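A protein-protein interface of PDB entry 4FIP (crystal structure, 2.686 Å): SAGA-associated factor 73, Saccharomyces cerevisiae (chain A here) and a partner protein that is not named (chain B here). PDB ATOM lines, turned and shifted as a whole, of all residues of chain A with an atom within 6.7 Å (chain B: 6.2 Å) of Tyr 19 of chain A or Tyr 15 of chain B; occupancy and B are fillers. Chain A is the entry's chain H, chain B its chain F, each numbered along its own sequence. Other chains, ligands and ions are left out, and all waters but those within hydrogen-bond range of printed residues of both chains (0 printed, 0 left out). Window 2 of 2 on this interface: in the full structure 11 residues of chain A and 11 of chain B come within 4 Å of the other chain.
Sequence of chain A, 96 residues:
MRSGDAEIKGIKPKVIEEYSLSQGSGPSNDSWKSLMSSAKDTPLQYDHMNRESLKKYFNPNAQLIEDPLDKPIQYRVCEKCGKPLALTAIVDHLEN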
ATOM      1  N   ILE A  11     -17.429 -23.380 -19.235  1.00  0.00           N
ATOM      2  CA  ILE A  11     -16.284 -23.574 -20.149  1.00  0.00           C
ATOM      3  C   ILE A  11     -15.471 -22.300 -20.329  1.00  0.00           C
ATOM      4  O   ILE A  11     -16.046 -21.220 -20.491  1.00  0.00           O
ATOM      5  CB  ILE A  11     -16.741 -24.026 -21.556  1.00  0.00           C
ATOM      6  CG1 ILE A  11     -16.807 -25.553 -21.642  1.00  0.00           C
ATOM      7  CG2 ILE A  11     -15.818 -23.480 -22.638  1.00  0.00           C
ATOM      8  CD1 ILE A  11     -17.856 -26.027 -22.620  1.00  0.00           C
ATOM      9  N   VAL A  15     -11.339 -21.657 -24.800  1.00  0.00           N
ATOM     10  CA  VAL A  15     -11.323 -23.037 -25.317  1.00  0.00           C
ATOM     11  C   VAL A  15     -12.322 -23.235 -26.465  1.00  0.00           C
ATOM     12  O   VAL A  15     -12.023 -23.958 -27.418  1.00  0.00           O
ATOM     13  CB  VAL A  15     -11.562 -24.111 -24.224  1.00  0.00           C
ATOM     14  CG1 VAL A  15     -10.566 -23.949 -23.083  1.00  0.00           C
ATOM     15  CG2 VAL A  15     -12.998 -24.081 -23.723  1.00  0.00           C
ATOM     16  N   ILE A  16     -13.481 -22.571 -26.407  1.00  0.00           N
ATOM     17  CA  ILE A  16     -14.479 -22.668 -27.493  1.00  0.00           C
ATOM     18  C   ILE A  16     -13.952 -21.986 -28.773  1.00  0.00           C
ATOM     19  O   ILE A  16     -14.732 -21.527 -29.600  1.00  0.00           O
ATOM     20  CB  ILE A  16     -15.866 -22.052 -27.128  1.00  0.00           C
ATOM     21  CG1 ILE A  16     -16.232 -22.221 -25.644  1.00  0.00           C
ATOM     22  CG2 ILE A  16     -16.955 -22.690 -27.982  1.00  0.00           C
ATOM     23  CD1 ILE A  16     -17.536 -21.553 -25.257  1.00  0.00           C
ATOM     24  N   GLU A  17     -12.625 -21.934 -28.922  1.00  0.00           N
ATOM     25  CA  GLU A  17     -11.948 -21.325 -30.070  1.00  0.00           C
ATOM     26  C   GLU A  17     -11.338 -22.394 -30.996  1.00  0.00           C
ATOM     27  O   GLU A  17     -11.099 -22.128 -32.175  1.00  0.00           O
ATOM     28  CB  GLU A  17     -10.850 -20.354 -29.591  1.00  0.00           C
ATOM     29  CG  GLU A  17     -11.264 -19.352 -28.504  1.00  0.00           C
ATOM     30  CD  GLU A  17     -11.984 -18.113 -29.031  1.00  0.00           C
ATOM     31  OE1 GLU A  17     -12.871 -18.238 -29.910  1.00  0.00           O
ATOM     32  OE2 GLU A  17     -11.670 -17.000 -28.551  1.00  0.00           O
ATOM     33  N   GLU A  18     -11.053 -23.579 -30.453  1.00  0.00           N
ATOM     34  CA  GLU A  18     -10.818 -24.787 -31.259  1.00  0.00           C
ATOM     35  C   GLU A  18     -12.069 -25.141 -32.082  1.00  0.00           C
ATOM     36  O   GLU A  18     -11.955 -25.659 -33.199  1.00  0.00           O
ATOM     37  CB  GLU A  18     -10.445 -25.963 -30.328  1.00  0.00           C
ATOM     38  CG  GLU A  18     -10.519 -27.378 -30.911  1.00  0.00           C
ATOM     39  CD  GLU A  18      -9.762 -28.403 -30.060  1.00  0.00           C
ATOM     40  OE1 GLU A  18     -10.397 -29.317 -29.497  1.00  0.00           O
ATOM     41  OE2 GLU A  18      -8.525 -28.302 -29.942  1.00  0.00           O
ATOM     42  N   TYR A  19     -13.244 -24.826 -31.515  1.00  0.00           N
ATOM     43  CA  TYR A  19     -14.569 -25.258 -32.004  1.00  0.00           C
ATOM     44  C   TYR A  19     -14.874 -24.821 -33.439  1.00  0.00           C
ATOM     45  O   TYR A  19     -14.396 -23.780 -33.901  1.00  0.00           O
ATOM     46  CB  TYR A  19     -15.663 -24.728 -31.047  1.00  0.00           C
ATOM     47  CG  TYR A  19     -17.064 -25.319 -31.195  1.00  0.00           C
ATOM     48  CD1 TYR A  19     -17.261 -26.658 -31.543  1.00  0.00           C
ATOM     49  CD2 TYR A  19     -18.195 -24.548 -30.926  1.00  0.00           C
ATOM     50  CE1 TYR A  19     -18.539 -27.194 -31.657  1.00  0.00           C
ATOM     51  CE2 TYR A  19     -19.476 -25.080 -31.031  1.00  0.00           C
ATOM     52  CZ  TYR A  19     -19.644 -26.402 -31.398  1.00  0.00           C
ATOM     53  OH  TYR A  19     -20.905 -26.946 -31.519  1.00  0.00           O
ATOM     54  N   SER A  20     -15.652 -25.648 -34.141  1.00  0.00           N
ATOM     55  CA  SER A  20     -16.181 -25.334 -35.481  1.00  0.00           C
ATOM     56  C   SER A  20     -17.232 -26.405 -35.916  1.00  0.00           C
ATOM     57  O   SER A  20     -16.929 -27.603 -35.933  1.00  0.00           O
ATOM     58  CB  SER A  20     -15.041 -25.224 -36.519  1.00  0.00           C
ATOM     59  OG  SER A  20     -14.130 -24.163 -36.237  1.00  0.00           O
ATOM     60  N   LEU A  21     -18.457 -25.973 -36.247  1.00  0.00           N
ATOM     61  CA  LEU A  21     -19.565 -26.890 -36.605  1.00  0.00           C
ATOM     62  C   LEU A  21     -20.583 -26.178 -37.487  1.00  0.00           C
ATOM     63  O   LEU A  21     -20.958 -25.042 -37.208  1.00  0.00           O
ATOM     64  CB  LEU A  21     -20.246 -27.442 -35.336  1.00  0.00           C
ATOM     65  CG  LEU A  21     -21.614 -28.140 -35.436  1.00  0.00           C
ATOM     66  CD1 LEU A  21     -21.710 -29.262 -34.412  1.00  0.00           C
ATOM     67  CD2 LEU A  21     -22.765 -27.156 -35.262  1.00  0.00           C
ATOM     68  N   SER B  10     -22.433 -32.422 -22.005  1.00  0.00           N
ATOM     69  CA  SER B  10     -22.314 -32.959 -23.356  1.00  0.00           C
ATOM     70  C   SER B  10     -21.231 -32.240 -24.157  1.00  0.00           C
ATOM     71  O   SER B  10     -20.562 -32.841 -25.010  1.00  0.00           O
ATOM     72  CB  SER B  10     -23.648 -32.789 -24.070  1.00  0.00           C
ATOM     73  OG  SER B  10     -24.133 -31.475 -23.870  1.00  0.00           O
ATOM     74  N   GLN B  11     -21.080 -30.951 -23.864  1.00  0.00           N
ATOM     75  CA  GLN B  11     -20.194 -30.049 -24.581  1.00  0.00           C
ATOM     76  C   GLN B  11     -18.746 -30.167 -24.069  1.00  0.00           C
ATOM     77  O   GLN B  11     -17.793 -29.911 -24.805  1.00  0.00           O
ATOM     78  CB  GLN B  11     -20.723 -28.606 -24.458  1.00  0.00           C
ATOM     79  CG  GLN B  11     -20.715 -27.843 -25.770  1.00  0.00           C
ATOM     80  CD  GLN B  11     -20.682 -26.343 -25.575  1.00  0.00           C
ATOM     81  OE1 GLN B  11     -20.997 -25.835 -24.492  1.00  0.00           O
ATOM     82  NE2 GLN B  11     -20.290 -25.618 -26.627  1.00  0.00           N
ATOM     83  N   ILE B  12     -18.582 -30.539 -22.802  1.00  0.00           N
ATOM     84  CA  ILE B  12     -17.276 -30.965 -22.292  1.00  0.00           C
ATOM     85  C   ILE B  12     -16.843 -32.207 -23.066  1.00  0.00           C
ATOM     86  O   ILE B  12     -15.753 -32.256 -23.653  1.00  0.00           O
ATOM     87  CB  ILE B  12     -17.352 -31.333 -20.797  1.00  0.00           C
ATOM     88  CG1 ILE B  12     -17.392 -30.069 -19.947  1.00  0.00           C
ATOM     89  CG2 ILE B  12     -16.191 -32.229 -20.388  1.00  0.00           C
ATOM     90  CD1 ILE B  12     -17.798 -30.331 -18.512  1.00  0.00           C
ATOM     91  N   GLN B  13     -17.726 -33.200 -23.059  1.00  0.00           N
ATOM     92  CA  GLN B  13     -17.514 -34.444 -23.777  1.00  0.00           C
ATOM     93  C   GLN B  13     -17.100 -34.184 -25.211  1.00  0.00           C
ATOM     94  O   GLN B  13     -16.128 -34.776 -25.678  1.00  0.00           O
ATOM     95  CB  GLN B  13     -18.763 -35.319 -23.702  1.00  0.00           C
ATOM     96  CG  GLN B  13     -18.908 -35.965 -22.333  1.00  0.00           C
ATOM     97  CD  GLN B  13     -20.112 -36.875 -22.224  1.00  0.00           C
ATOM     98  OE1 GLN B  13     -19.973 -38.084 -22.023  1.00  0.00           O
ATOM     99  NE2 GLN B  13     -21.296 -36.306 -22.361  1.00  0.00           N
ATOM    100  N   GLN B  14     -17.796 -33.273 -25.887  1.00  0.00           N
ATOM    101  CA  GLN B  14     -17.437 -32.895 -27.253  1.00  0.00           C
ATOM    102  C   GLN B  14     -15.969 -32.494 -27.359  1.00  0.00           C
ATOM    103  O   GLN B  14     -15.266 -32.959 -28.243  1.00  0.00           O
ATOM    104  CB  GLN B  14     -18.322 -31.759 -27.767  1.00  0.00           C
ATOM    105  CG  GLN B  14     -19.718 -32.180 -28.211  1.00  0.00           C
ATOM    106  CD  GLN B  14     -20.744 -31.051 -28.132  1.00  0.00           C
ATOM    107  OE1 GLN B  14     -21.934 -31.310 -27.928  1.00  0.00           O
ATOM    108  NE2 GLN B  14     -20.294 -29.794 -28.289  1.00  0.00           N
ATOM    109  N   TYR B  15     -15.482 -31.656 -26.454  1.00  0.00           N
ATOM    110  CA  TYR B  15     -14.104 -31.162 -26.592  1.00  0.00           C
ATOM    111  C   TYR B  15     -13.078 -32.248 -26.222  1.00  0.00           C
ATOM    112  O   TYR B  15     -12.034 -32.378 -26.868  1.00  0.00           O
ATOM    113  CB  TYR B  15     -13.910 -29.826 -25.847  1.00  0.00           C
ATOM    114  CG  TYR B  15     -14.926 -28.739 -26.281  1.00  0.00           C
ATOM    115  CD1 TYR B  15     -15.263 -28.542 -27.636  1.00  0.00           C
ATOM    116  CD2 TYR B  15     -15.555 -27.918 -25.343  1.00  0.00           C
ATOM    117  CE1 TYR B  15     -16.192 -27.577 -28.029  1.00  0.00           C
ATOM    118  CE2 TYR B  15     -16.481 -26.942 -25.735  1.00  0.00           C
ATOM    119  CZ  TYR B  15     -16.800 -26.775 -27.074  1.00  0.00           C
ATOM    120  OH  TYR B  15     -17.723 -25.804 -27.452  1.00  0.00           O
ATOM    121  N   LEU B  16     -13.405 -33.077 -25.239  1.00  0.00           N
ATOM    122  CA  LEU B  16     -12.576 -34.243 -24.946  1.00  0.00           C
ATOM    123  C   LEU B  16     -12.380 -35.116 -26.188  1.00  0.00           C
ATOM    124  O   LEU B  16     -11.248 -35.426 -26.582  1.00  0.00           O
ATOM    125  CB  LEU B  16     -13.199 -35.076 -23.833  1.00  0.00           C
ATOM    126  CG  LEU B  16     -13.091 -34.436 -22.458  1.00  0.00           C
ATOM    127  CD1 LEU B  16     -13.942 -35.185 -21.447  1.00  0.00           C
ATOM    128  CD2 LEU B  16     -11.649 -34.404 -22.006  1.00  0.00           C
ATOM    129  N   VAL B  17     -13.487 -35.503 -26.810  1.00  0.00           N
ATOM    130  CA  VAL B  17     -13.409 -36.316 -28.015  1.00  0.00           C
ATOM    131  C   VAL B  17     -12.584 -35.573 -29.059  1.00  0.00           C
ATOM    132  O   VAL B  17     -11.573 -36.076 -29.530  1.00  0.00           O
ATOM    133  CB  VAL B  17     -14.809 -36.697 -28.540  1.00  0.00           C
ATOM    134  CG1 VAL B  17     -14.727 -37.376 -29.901  1.00  0.00           C
ATOM    135  CG2 VAL B  17     -15.506 -37.606 -27.529  1.00  0.00           C
ATOM    136  N   GLU B  18     -12.962 -34.340 -29.352  1.00  0.00           N
ATOM    137  CA  GLU B  18     -12.258 -33.553 -30.372  1.00  0.00           C
ATOM    138  C   GLU B  18     -10.755 -33.280 -30.085  1.00  0.00           C
ATOM    139  O   GLU B  18      -9.944 -33.218 -31.015  1.00  0.00           O
ATOM    140  CB  GLU B  18     -13.052 -32.272 -30.677  1.00  0.00           C
ATOM    141  CG  GLU B  18     -14.268 -32.545 -31.585  1.00  0.00           C
ATOM    142  CD  GLU B  18     -15.442 -31.572 -31.419  1.00  0.00           C
ATOM    143  OE1 GLU B  18     -16.518 -31.841 -32.010  1.00  0.00           O
ATOM    144  OE2 GLU B  18     -15.312 -30.550 -30.710  1.00  0.00           O
ATOM    145  N   SER B  19     -10.361 -33.164 -28.821  1.00  0.00           N
ATOM    146  CA  SER B  19      -8.927 -33.083 -28.498  1.00  0.00           C
ATOM    147  C   SER B  19      -8.190 -34.444 -28.572  1.00  0.00           C
ATOM    148  O   SER B  19      -6.987 -34.483 -28.839  1.00  0.00           O
ATOM    149  CB  SER B  19      -8.758 -32.529 -27.108  1.00  0.00           C
ATOM    150  OG  SER B  19      -9.198 -33.489 -26.167  1.00  0.00           O
ATOM    151  N   GLY B  20      -8.903 -35.548 -28.302  1.00  0.00           N
ATOM    152  CA  GLY B  20      -8.316 -36.901 -28.305  1.00  0.00           C
ATOM    153  C   GLY B  20      -8.187 -37.530 -26.934  1.00  0.00           C
ATOM    154  O   GLY B  20      -7.810 -38.673 -26.805  1.00  0.00           O
ATOM    155  N   ASN B  21      -8.514 -36.775 -25.909  1.00  0.00           N
ATOM    156  CA  ASN B  21      -8.368 -37.218 -24.533  1.00  0.00           C
ATOM    157  C   ASN B  21      -9.493 -38.152 -24.121  1.00  0.00           C
ATOM    158  O   ASN B  21      -9.391 -38.867 -23.106  1.00  0.00           O
ATOM    159  CB  ASN B  21      -8.372 -36.002 -23.602  1.00  0.00           C
ATOM    160  CG  ASN B  21      -7.291 -34.985 -23.954  1.00  0.00           C
ATOM    161  OD1 ASN B  21      -7.292 -33.878 -23.437  1.00  0.00           O
ATOM    162  ND2 ASN B  21      -6.359 -35.362 -24.830  1.00  0.00           N
ATOM    163  N   ILE B  92      -9.674 -27.165 -19.553  1.00  0.00           N
ATOM    164  CA  ILE B  92     -10.716 -26.476 -20.365  1.00  0.00           C
ATOM    165  C   ILE B  92     -11.913 -25.845 -19.596  1.00  0.00           C
ATOM    166  O   ILE B  92     -12.574 -24.953 -20.121  1.00  0.00           O
ATOM    167  CB  ILE B  92     -11.247 -27.411 -21.486  1.00  0.00           C
ATOM    168  CG1 ILE B  92     -12.189 -28.488 -20.921  1.00  0.00           C
ATOM    169  CG2 ILE B  92     -10.074 -28.037 -22.235  1.00  0.00           C
ATOM    170  CD1 ILE B  92     -12.364 -29.690 -21.829  1.00  0.00           C
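Tyr 19 of chain A touches one residue of chain B. Of chain A, only Ile 11 (3.5 Å), Ile 16 (3.3 Å) and Tyr 19 (3.7 Å) come within 4 Å of Tyr 15 of chain B. Of the printed residues of chain A, Gln 11 of chain B touches Ile 11. Of the printed residues of chain B, Ile 16 of chain A touches Tyr 15 (3.3 Å). Printed residues of chain A within 4 Å of Ser 19 of chain B: Glu 18. Of the printed residues of chain B, Ile 11 of chain A touches Gln 11, Tyr 15 and Ile 92. Printed residues of chain B within 4 Å of Glu 18 of chain A: Ser 19 (3.9 Å). Ile 12 of chain B touches none of the printed residues of chain A. Leu 21 of chain A touches none of the printed residues of chain B. The nearest residue of chain B that does not touch Tyr 19 of chain A is Gln 14 of chain B (4.3 Å). The nearest printed residue of chain B that does not touch Glu 18 of chain A is Glu 18 of chain B (4.02 Å).
OG of Ser 19 of chain B is in hydrogen-bond range of O of Leu 16 of chain B (2.9 Å). The side-chain hydroxyl (OG) of Ser 19 of chain B is in hydrogen-bond range of the backbone carbonyl oxygen (O) of Tyr 15 of chain B (3.1 Å). NE2 of Gln 11 of chain B lies within hydrogen-bond range of OH of Tyr 15 of chain B, at 2.7 Å. The side-chain hydroxyl of Ser 19 of chain B lies close to the side-chain amide oxygen of Asn 21 of chain B, at 3.4 Å.
Of the 13 printed residues of chain B, 4 touch a printed residue of chain A.
Among the printed residues, pairs that only touch across the chains: Ile 11 of chain A with Gln 11 of chain B, Ile 11 of chain A with Tyr 15 of chain B, Ile 11 of chain A with Ile 92 of chain B, Val 15 of chain A with Ile 92 of chain B, Ile 16 of chain A with Tyr 15 of chain B, Glu 18 of chain A with Ser 19 of chain B and Tyr 19 of chain A with Tyr 15 of chain B.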
